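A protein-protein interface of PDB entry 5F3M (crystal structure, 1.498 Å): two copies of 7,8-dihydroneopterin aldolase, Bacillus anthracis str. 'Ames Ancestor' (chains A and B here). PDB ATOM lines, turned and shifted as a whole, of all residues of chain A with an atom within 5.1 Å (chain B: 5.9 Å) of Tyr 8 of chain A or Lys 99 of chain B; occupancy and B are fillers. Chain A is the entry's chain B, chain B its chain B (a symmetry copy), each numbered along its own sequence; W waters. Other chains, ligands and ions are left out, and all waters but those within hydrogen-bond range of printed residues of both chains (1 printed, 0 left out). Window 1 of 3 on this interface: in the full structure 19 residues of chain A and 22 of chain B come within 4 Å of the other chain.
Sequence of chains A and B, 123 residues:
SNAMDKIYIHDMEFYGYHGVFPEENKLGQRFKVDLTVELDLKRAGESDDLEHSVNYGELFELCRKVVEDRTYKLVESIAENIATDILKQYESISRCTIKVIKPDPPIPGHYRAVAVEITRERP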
ATOM      1  N   LYS A   6     -13.083   1.674 -18.579  1.00  0.00           N
ATOM      2  CA  LYS A   6     -12.238   2.807 -18.221  1.00  0.00           C
ATOM      3  C   LYS A   6     -12.245   3.889 -19.287  1.00  0.00           C
ATOM      4  O   LYS A   6     -12.293   3.603 -20.488  1.00  0.00           O
ATOM      5  CB  LYS A   6     -10.788   2.363 -17.983  1.00  0.00           C
ATOM      6  CG  LYS A   6     -10.657   1.464 -16.762  1.00  0.00           C
ATOM      7  CD  LYS A   6      -9.289   0.849 -16.625  1.00  0.00           C
ATOM      8  CE  LYS A   6      -9.279  -0.120 -15.460  1.00  0.00           C
ATOM      9  NZ  LYS A   6     -10.106  -1.334 -15.743  1.00  0.00           N
ATOM     10  N   ILE A   7     -12.176   5.138 -18.835  1.00  0.00           N
ATOM     11  CA  ILE A   7     -11.750   6.254 -19.673  1.00  0.00           C
ATOM     12  C   ILE A   7     -10.354   6.654 -19.220  1.00  0.00           C
ATOM     13  O   ILE A   7     -10.090   6.746 -18.011  1.00  0.00           O
ATOM     14  CB  ILE A   7     -12.714   7.452 -19.570  1.00  0.00           C
ATOM     15  CG1 ILE A   7     -14.068   7.114 -20.186  1.00  0.00           C
ATOM     16  CG2 ILE A   7     -12.112   8.694 -20.244  1.00  0.00           C
ATOM     17  CD1 ILE A   7     -15.154   8.098 -19.800  1.00  0.00           C
ATOM     18  N   TYR A   8      -9.457   6.884 -20.185  1.00  0.00           N
ATOM     19  CA  TYR A   8      -8.105   7.353 -19.917  1.00  0.00           C
ATOM     20  C   TYR A   8      -7.865   8.717 -20.558  1.00  0.00           C
ATOM     21  O   TYR A   8      -8.346   9.002 -21.660  1.00  0.00           O
ATOM     22  CB  TYR A   8      -7.063   6.427 -20.548  1.00  0.00           C
ATOM     23  CG  TYR A   8      -6.992   5.016 -20.017  1.00  0.00           C
ATOM     24  CD1 TYR A   8      -6.408   4.743 -18.787  1.00  0.00           C
ATOM     25  CD2 TYR A   8      -7.459   3.946 -20.777  1.00  0.00           C
ATOM     26  CE1 TYR A   8      -6.308   3.436 -18.314  1.00  0.00           C
ATOM     27  CE2 TYR A   8      -7.364   2.642 -20.317  1.00  0.00           C
ATOM     28  CZ  TYR A   8      -6.787   2.397 -19.082  1.00  0.00           C
ATOM     29  OH  TYR A   8      -6.677   1.102 -18.628  1.00  0.00           O
ATOM     30  N   ILE A   9      -7.076   9.545 -19.879  1.00  0.00           N
ATOM     31  CA  ILE A   9      -6.385  10.662 -20.519  1.00  0.00           C
ATOM     32  C   ILE A   9      -4.907  10.497 -20.203  1.00  0.00           C
ATOM     33  O   ILE A   9      -4.514  10.521 -19.026  1.00  0.00           O
ATOM     34  CB  ILE A   9      -6.897  12.041 -20.067  1.00  0.00           C
ATOM     35  CG1 ILE A   9      -8.412  12.139 -20.253  1.00  0.00           C
ATOM     36  CG2 ILE A   9      -6.210  13.130 -20.885  1.00  0.00           C
ATOM     37  CD1 ILE A   9      -8.989  13.474 -19.766  1.00  0.00           C
ATOM     38  N   HIS A  10      -4.090  10.329 -21.241  1.00  0.00           N
ATOM     39  CA  HIS A  10      -2.686   9.975 -21.088  1.00  0.00           C
ATOM     40  C   HIS A  10      -1.781  11.195 -21.236  1.00  0.00           C
ATOM     41  O   HIS A  10      -1.873  11.933 -22.229  1.00  0.00           O
ATOM     42  CB  HIS A  10      -2.266   8.972 -22.165  1.00  0.00           C
ATOM     43  CG  HIS A  10      -2.904   7.624 -22.051  1.00  0.00           C
ATOM     44  ND1 HIS A  10      -3.148   7.006 -20.843  1.00  0.00           N
ATOM     45  CD2 HIS A  10      -3.317   6.756 -23.006  1.00  0.00           C
ATOM     46  CE1 HIS A  10      -3.692   5.821 -21.058  1.00  0.00           C
ATOM     47  NE2 HIS A  10      -3.805   5.645 -22.362  1.00  0.00           N
ATOM     48  N   LEU A  35      -4.646  10.092 -16.108  1.00  0.00           N
ATOM     49  CA  LEU A  35      -5.947   9.905 -15.478  1.00  0.00           C
ATOM     50  C   LEU A  35      -6.561   8.598 -15.953  1.00  0.00           C
ATOM     51  O   LEU A  35      -6.539   8.295 -17.148  1.00  0.00           O
ATOM     52  CB  LEU A  35      -6.889  11.077 -15.807  1.00  0.00           C
ATOM     53  CG  LEU A  35      -8.384  10.978 -15.440  1.00  0.00           C
ATOM     54  CD1 LEU A  35      -8.952  12.377 -15.201  1.00  0.00           C
ATOM     55  CD2 LEU A  35      -9.214  10.272 -16.511  1.00  0.00           C
ATOM     56  N   THR A  36      -7.116   7.834 -15.008  1.00  0.00           N
ATOM     57  CA  THR A  36      -7.976   6.689 -15.291  1.00  0.00           C
ATOM     58  C   THR A  36      -9.232   6.849 -14.448  1.00  0.00           C
ATOM     59  O   THR A  36      -9.137   7.070 -13.238  1.00  0.00           O
ATOM     60  CB  THR A  36      -7.298   5.376 -14.867  1.00  0.00           C
ATOM     61  OG1 THR A  36      -6.018   5.242 -15.500  1.00  0.00           O
ATOM     62  CG2 THR A  36      -8.178   4.168 -15.217  1.00  0.00           C
ATOM     63  N   LYS B  32      -6.759   5.075 -33.088  1.00  0.00           N
ATOM     64  CA  LYS B  32      -5.901   3.927 -32.855  1.00  0.00           C
ATOM     65  C   LYS B  32      -6.666   2.897 -32.038  1.00  0.00           C
ATOM     66  O   LYS B  32      -7.569   3.239 -31.267  1.00  0.00           O
ATOM     67  CB  LYS B  32      -4.606   4.329 -32.134  1.00  0.00           C
ATOM     68  CG  LYS B  32      -3.739   5.339 -32.912  1.00  0.00           C
ATOM     69  CD  LYS B  32      -2.593   5.836 -32.035  1.00  0.00           C
ATOM     70  CE  LYS B  32      -1.343   6.158 -32.847  1.00  0.00           C
ATOM     71  NZ  LYS B  32      -1.589   7.184 -33.897  1.00  0.00           N
ATOM     72  N   VAL B  33      -6.322   1.627 -32.223  1.00  0.00           N
ATOM     73  CA  VAL B  33      -6.961   0.538 -31.490  1.00  0.00           C
ATOM     74  C   VAL B  33      -5.888  -0.425 -30.999  1.00  0.00           C
ATOM     75  O   VAL B  33      -5.005  -0.820 -31.768  1.00  0.00           O
ATOM     76  CB  VAL B  33      -7.995  -0.211 -32.357  1.00  0.00           C
ATOM     77  CG1 VAL B  33      -8.651  -1.338 -31.555  1.00  0.00           C
ATOM     78  CG2 VAL B  33      -9.060   0.731 -32.891  1.00  0.00           C
ATOM     79  N   ASP B  34      -5.974  -0.815 -29.726  1.00  0.00           N
ATOM     80  CA  ASP B  34      -5.226  -1.950 -29.200  1.00  0.00           C
ATOM     81  C   ASP B  34      -6.226  -3.071 -28.958  1.00  0.00           C
ATOM     82  O   ASP B  34      -7.282  -2.841 -28.356  1.00  0.00           O
ATOM     83  CB  ASP B  34      -4.556  -1.626 -27.860  1.00  0.00           C
ATOM     84  CG  ASP B  34      -3.422  -0.619 -27.974  1.00  0.00           C
ATOM     85  OD1 ASP B  34      -2.810  -0.474 -29.052  1.00  0.00           O
ATOM     86  OD2 ASP B  34      -3.124   0.025 -26.943  1.00  0.00           O
ATOM     87  N   LEU B  35      -5.896  -4.272 -29.418  1.00  0.00           N
ATOM     88  CA  LEU B  35      -6.754  -5.439 -29.266  1.00  0.00           C
ATOM     89  C   LEU B  35      -6.038  -6.494 -28.439  1.00  0.00           C
ATOM     90  O   LEU B  35      -4.858  -6.771 -28.663  1.00  0.00           O
ATOM     91  CB  LEU B  35      -7.137  -6.021 -30.639  1.00  0.00           C
ATOM     92  CG  LEU B  35      -7.846  -7.389 -30.715  1.00  0.00           C
ATOM     93  CD1 LEU B  35      -8.713  -7.453 -31.972  1.00  0.00           C
ATOM     94  CD2 LEU B  35      -6.870  -8.565 -30.712  1.00  0.00           C
ATOM     95  N   ALA B  79     -15.526   0.777 -29.554  1.00  0.00           N
ATOM     96  CA  ALA B  79     -15.050  -0.315 -28.707  1.00  0.00           C
ATOM     97  C   ALA B  79     -16.114  -1.394 -28.550  1.00  0.00           C
ATOM     98  O   ALA B  79     -15.831  -2.590 -28.687  1.00  0.00           O
ATOM     99  CB  ALA B  79     -14.633   0.234 -27.340  1.00  0.00           C
ATOM    100  N   THR B  97     -10.336  -7.542 -24.662  1.00  0.00           N
ATOM    101  CA  THR B  97     -10.158  -6.184 -24.164  1.00  0.00           C
ATOM    102  C   THR B  97      -9.835  -5.295 -25.355  1.00  0.00           C
ATOM    103  O   THR B  97      -8.854  -5.539 -26.069  1.00  0.00           O
ATOM    104  CB  THR B  97      -9.040  -6.113 -23.121  1.00  0.00           C
ATOM    105  OG1 THR B  97      -9.407  -6.905 -21.988  1.00  0.00           O
ATOM    106  CG2 THR B  97      -8.837  -4.684 -22.661  1.00  0.00           C
ATOM    107  N   ILE B  98     -10.647  -4.265 -25.558  1.00  0.00           N
ATOM    108  CA  ILE B  98     -10.514  -3.369 -26.701  1.00  0.00           C
ATOM    109  C   ILE B  98     -10.274  -1.970 -26.166  1.00  0.00           C
ATOM    110  O   ILE B  98     -11.079  -1.459 -25.374  1.00  0.00           O
ATOM    111  CB  ILE B  98     -11.763  -3.400 -27.597  1.00  0.00           C
ATOM    112  CG1 ILE B  98     -12.074  -4.841 -28.043  1.00  0.00           C
ATOM    113  CG2 ILE B  98     -11.575  -2.474 -28.807  1.00  0.00           C
ATOM    114  CD1 ILE B  98     -10.928  -5.498 -28.815  1.00  0.00           C
ATOM    115  N   LYS B  99      -9.174  -1.352 -26.592  1.00  0.00           N
ATOM    116  CA  LYS B  99      -8.863   0.029 -26.248  1.00  0.00           C
ATOM    117  C   LYS B  99      -8.938   0.848 -27.529  1.00  0.00           C
ATOM    118  O   LYS B  99      -8.258   0.527 -28.513  1.00  0.00           O
ATOM    119  CB  LYS B  99      -7.472   0.139 -25.621  1.00  0.00           C
ATOM    120  CG  LYS B  99      -7.142   1.533 -25.128  1.00  0.00           C
ATOM    121  CD  LYS B  99      -5.740   1.599 -24.547  1.00  0.00           C
ATOM    122  CE  LYS B  99      -5.420   2.986 -24.008  1.00  0.00           C
ATOM    123  NZ  LYS B  99      -4.029   3.007 -23.462  1.00  0.00           N
ATOM    124  N   VAL B 100      -9.783   1.879 -27.532  1.00  0.00           N
ATOM    125  CA  VAL B 100      -9.914   2.783 -28.673  1.00  0.00           C
ATOM    126  C   VAL B 100      -9.347   4.135 -28.260  1.00  0.00           C
ATOM    127  O   VAL B 100      -9.775   4.717 -27.252  1.00  0.00           O
ATOM    128  CB  VAL B 100     -11.366   2.900 -29.159  1.00  0.00           C
ATOM    129  CG1 VAL B 100     -11.466   3.888 -30.310  1.00  0.00           C
ATOM    130  CG2 VAL B 100     -11.902   1.528 -29.569  1.00  0.00           C
ATOM    131  N   ILE B 101      -8.386   4.624 -29.043  1.00  0.00           N
ATOM    132  CA  ILE B 101      -7.589   5.793 -28.706  1.00  0.00           C
ATOM    133  C   ILE B 101      -7.873   6.889 -29.720  1.00  0.00           C
ATOM    134  O   ILE B 101      -7.851   6.650 -30.931  1.00  0.00           O
ATOM    135  CB  ILE B 101      -6.086   5.455 -28.695  1.00  0.00           C
ATOM    136  CG1 ILE B 101      -5.811   4.321 -27.702  1.00  0.00           C
ATOM    137  CG2 ILE B 101      -5.264   6.700 -28.373  1.00  0.00           C
ATOM    138  CD1 ILE B 101      -5.242   3.080 -28.347  1.00  0.00           C
ATOM    139  N   ALA B 113      -3.134  11.602 -25.567  1.00  0.00           N
ATOM    140  CA  ALA B 113      -4.325  10.981 -26.142  1.00  0.00           C
ATOM    141  C   ALA B 113      -5.416  10.875 -25.091  1.00  0.00           C
ATOM    142  O   ALA B 113      -5.151  10.933 -23.889  1.00  0.00           O
ATOM    143  CB  ALA B 113      -4.024   9.567 -26.666  1.00  0.00           C
ATOM    144  N   VAL B 114      -6.648  10.707 -25.571  1.00  0.00           N
ATOM    145  CA  VAL B 114      -7.759  10.222 -24.758  1.00  0.00           C
ATOM    146  C   VAL B 114      -8.130   8.833 -25.270  1.00  0.00           C
ATOM    147  O   VAL B 114      -7.857   8.483 -26.418  1.00  0.00           O
ATOM    148  CB  VAL B 114      -8.977  11.173 -24.784  1.00  0.00           C
ATOM    149  CG1 VAL B 114      -8.575  12.578 -24.328  1.00  0.00           C
ATOM    150  CG2 VAL B 114      -9.617  11.202 -26.171  1.00  0.00           C
ATOM    151  N   ALA B 115      -8.755   8.025 -24.408  1.00  0.00           N
ATOM    152  CA  ALA B 115      -9.047   6.649 -24.804  1.00  0.00           C
ATOM    153  C   ALA B 115     -10.159   6.072 -23.944  1.00  0.00           C
ATOM    154  O   ALA B 115     -10.417   6.534 -22.829  1.00  0.00           O
ATOM    155  CB  ALA B 115      -7.819   5.740 -24.689  1.00  0.00           C
ATOM    156  N   VAL B 116     -10.813   5.042 -24.484  1.00  0.00           N
ATOM    157  CA  VAL B 116     -11.718   4.198 -23.715  1.00  0.00           C
ATOM    158  C   VAL B 116     -11.224   2.762 -23.806  1.00  0.00           C
ATOM    159  O   VAL B 116     -10.613   2.356 -24.800  1.00  0.00           O
ATOM    160  CB  VAL B 116     -13.193   4.285 -24.168  1.00  0.00           C
ATOM    161  CG1 VAL B 116     -13.751   5.690 -23.971  1.00  0.00           C
ATOM    162  CG2 VAL B 116     -13.354   3.793 -25.599  1.00  0.00           C
ATOM    163  N   GLU B 117     -11.519   1.978 -22.770  1.00  0.00           N
ATOM    164  CA  GLU B 117     -11.111   0.581 -22.764  1.00  0.00           C
ATOM    165  C   GLU B 117     -12.193  -0.256 -22.107  1.00  0.00           C
ATOM    166  O   GLU B 117     -12.657   0.075 -21.013  1.00  0.00           O
ATOM    167  CB  GLU B 117      -9.795   0.420 -22.009  1.00  0.00           C
ATOM    168  CG  GLU B 117      -9.224  -0.972 -22.007  1.00  0.00           C
ATOM    169  CD  GLU B 117      -7.898  -0.990 -21.293  1.00  0.00           C
ATOM    170  OE1 GLU B 117      -7.891  -0.899 -20.045  1.00  0.00           O
ATOM    171  OE2 GLU B 117      -6.865  -1.030 -21.984  1.00  0.00           O
ATOM    172  N   ILE B 118     -12.599  -1.331 -22.778  1.00  0.00           N
ATOM    173  CA  ILE B 118     -13.615  -2.228 -22.248  1.00  0.00           C
ATOM    174  C   ILE B 118     -13.122  -3.665 -22.314  1.00  0.00           C
ATOM    175  O   ILE B 118     -12.331  -4.038 -23.185  1.00  0.00           O
ATOM    176  CB  ILE B 118     -14.972  -2.087 -22.978  1.00  0.00           C
ATOM    177  CG1 ILE B 118     -14.883  -2.625 -24.416  1.00  0.00           C
ATOM    178  CG2 ILE B 118     -15.472  -0.635 -22.929  1.00  0.00           C
ATOM    179  CD1 ILE B 118     -16.202  -2.547 -25.171  1.00  0.00           C
HETATM  180  O   HOH W   1      -9.169  -2.257 -18.224  1.00  0.00           O
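Tyr 8 of chain A touches just these residues of chain B: Lys 99 (3.9 Å), Val 114 (3.4 Å), Ala 115 (2.8 Å) and Glu 117 (2.7 Å). Lys 99 of chain B touches just these residues of chain A: Tyr 8 and His 10. Of the printed residues of chain A, Glu 117 of chain B touches Lys 6 and Tyr 8. Of the printed residues of chain A, Val 116 of chain B touches Lys 6 (3.3 Å). Printed residues of chain B within 4 Å of His 10 of chain A: Lys 99 and Ala 113. Printed residues of chain A within 4 Å of Val 114 of chain B: Tyr 8 (3.4 Å). Of the printed residues of chain A, Ala 113 of chain B touches Ile 9 and His 10. Ala 79 of chain B touches none of the printed residues of chain A. The nearest residue of chain B that does not touch Tyr 8 of chain A is Ala 113 of chain B (4.3 Å). The nearest printed residue of chain A that does not touch Lys 99 of chain B is Lys 6 of chain A (7.2 Å). The nearest printed residue of chain A that does not touch Val 114 of chain B is Ile 9 of chain A (4.1 Å).
Among the printed residues, pairs that only touch across the chains: Lys 6 of chain A with Val 116 of chain B, Tyr 8 of chain A with Val 114 of chain B, Ile 7 of chain A with Ala 115 of chain B, Ile 9 of chain A with Ala 113 of chain B and Tyr 8 of chain A with Lys 99 of chain B.
Position printed for both chains: 35.
The backbone NH of Leu 35 of chain A sits at hydrogen-bond distance from the backbone carbonyl oxygen of Ile 9 of chain A. The backbone NH (N) of Asp 34 of chain B lies within hydrogen-bond range of the backbone carbonyl oxygen (O) of Lys 99 of chain B (2.9 Å). N of Val 100 of chain B sits at hydrogen-bond distance from O of Val 116 of chain B (2.9 Å).
Water W1 bridges OE1 of Glu 117 of chain B and NZ of Lys 6 of chain A.
Hydrophobic or aromatic side chains of chain B within 4 Å of the printed part of chain A: Val 114 and Val 116. Hydrophobic or aromatic side chains of chain A within 4 Å of the printed part of chain B: Ile 7, Tyr 8, Ile 9 and His 10.
O of Lys 6 of chain A lies within hydrogen-bond range of N of Glu 117 of chain B. The backbone NH of Tyr 8 of chain A sits at hydrogen-bond distance from the backbone carbonyl oxygen of Ala 115 of chain B. OH of Tyr 8 of chain A sits at hydrogen-bond distance from OE1 of Glu 117 of chain B (2.7 Å). NZ of Lys 99 of chain B sits at hydrogen-bond distance from NE2 of His 10 of chain A (2.9 Å). O of Ala 113 of chain B lies within hydrogen-bond range of N of His 10 of chain A, 2.9 Å away.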
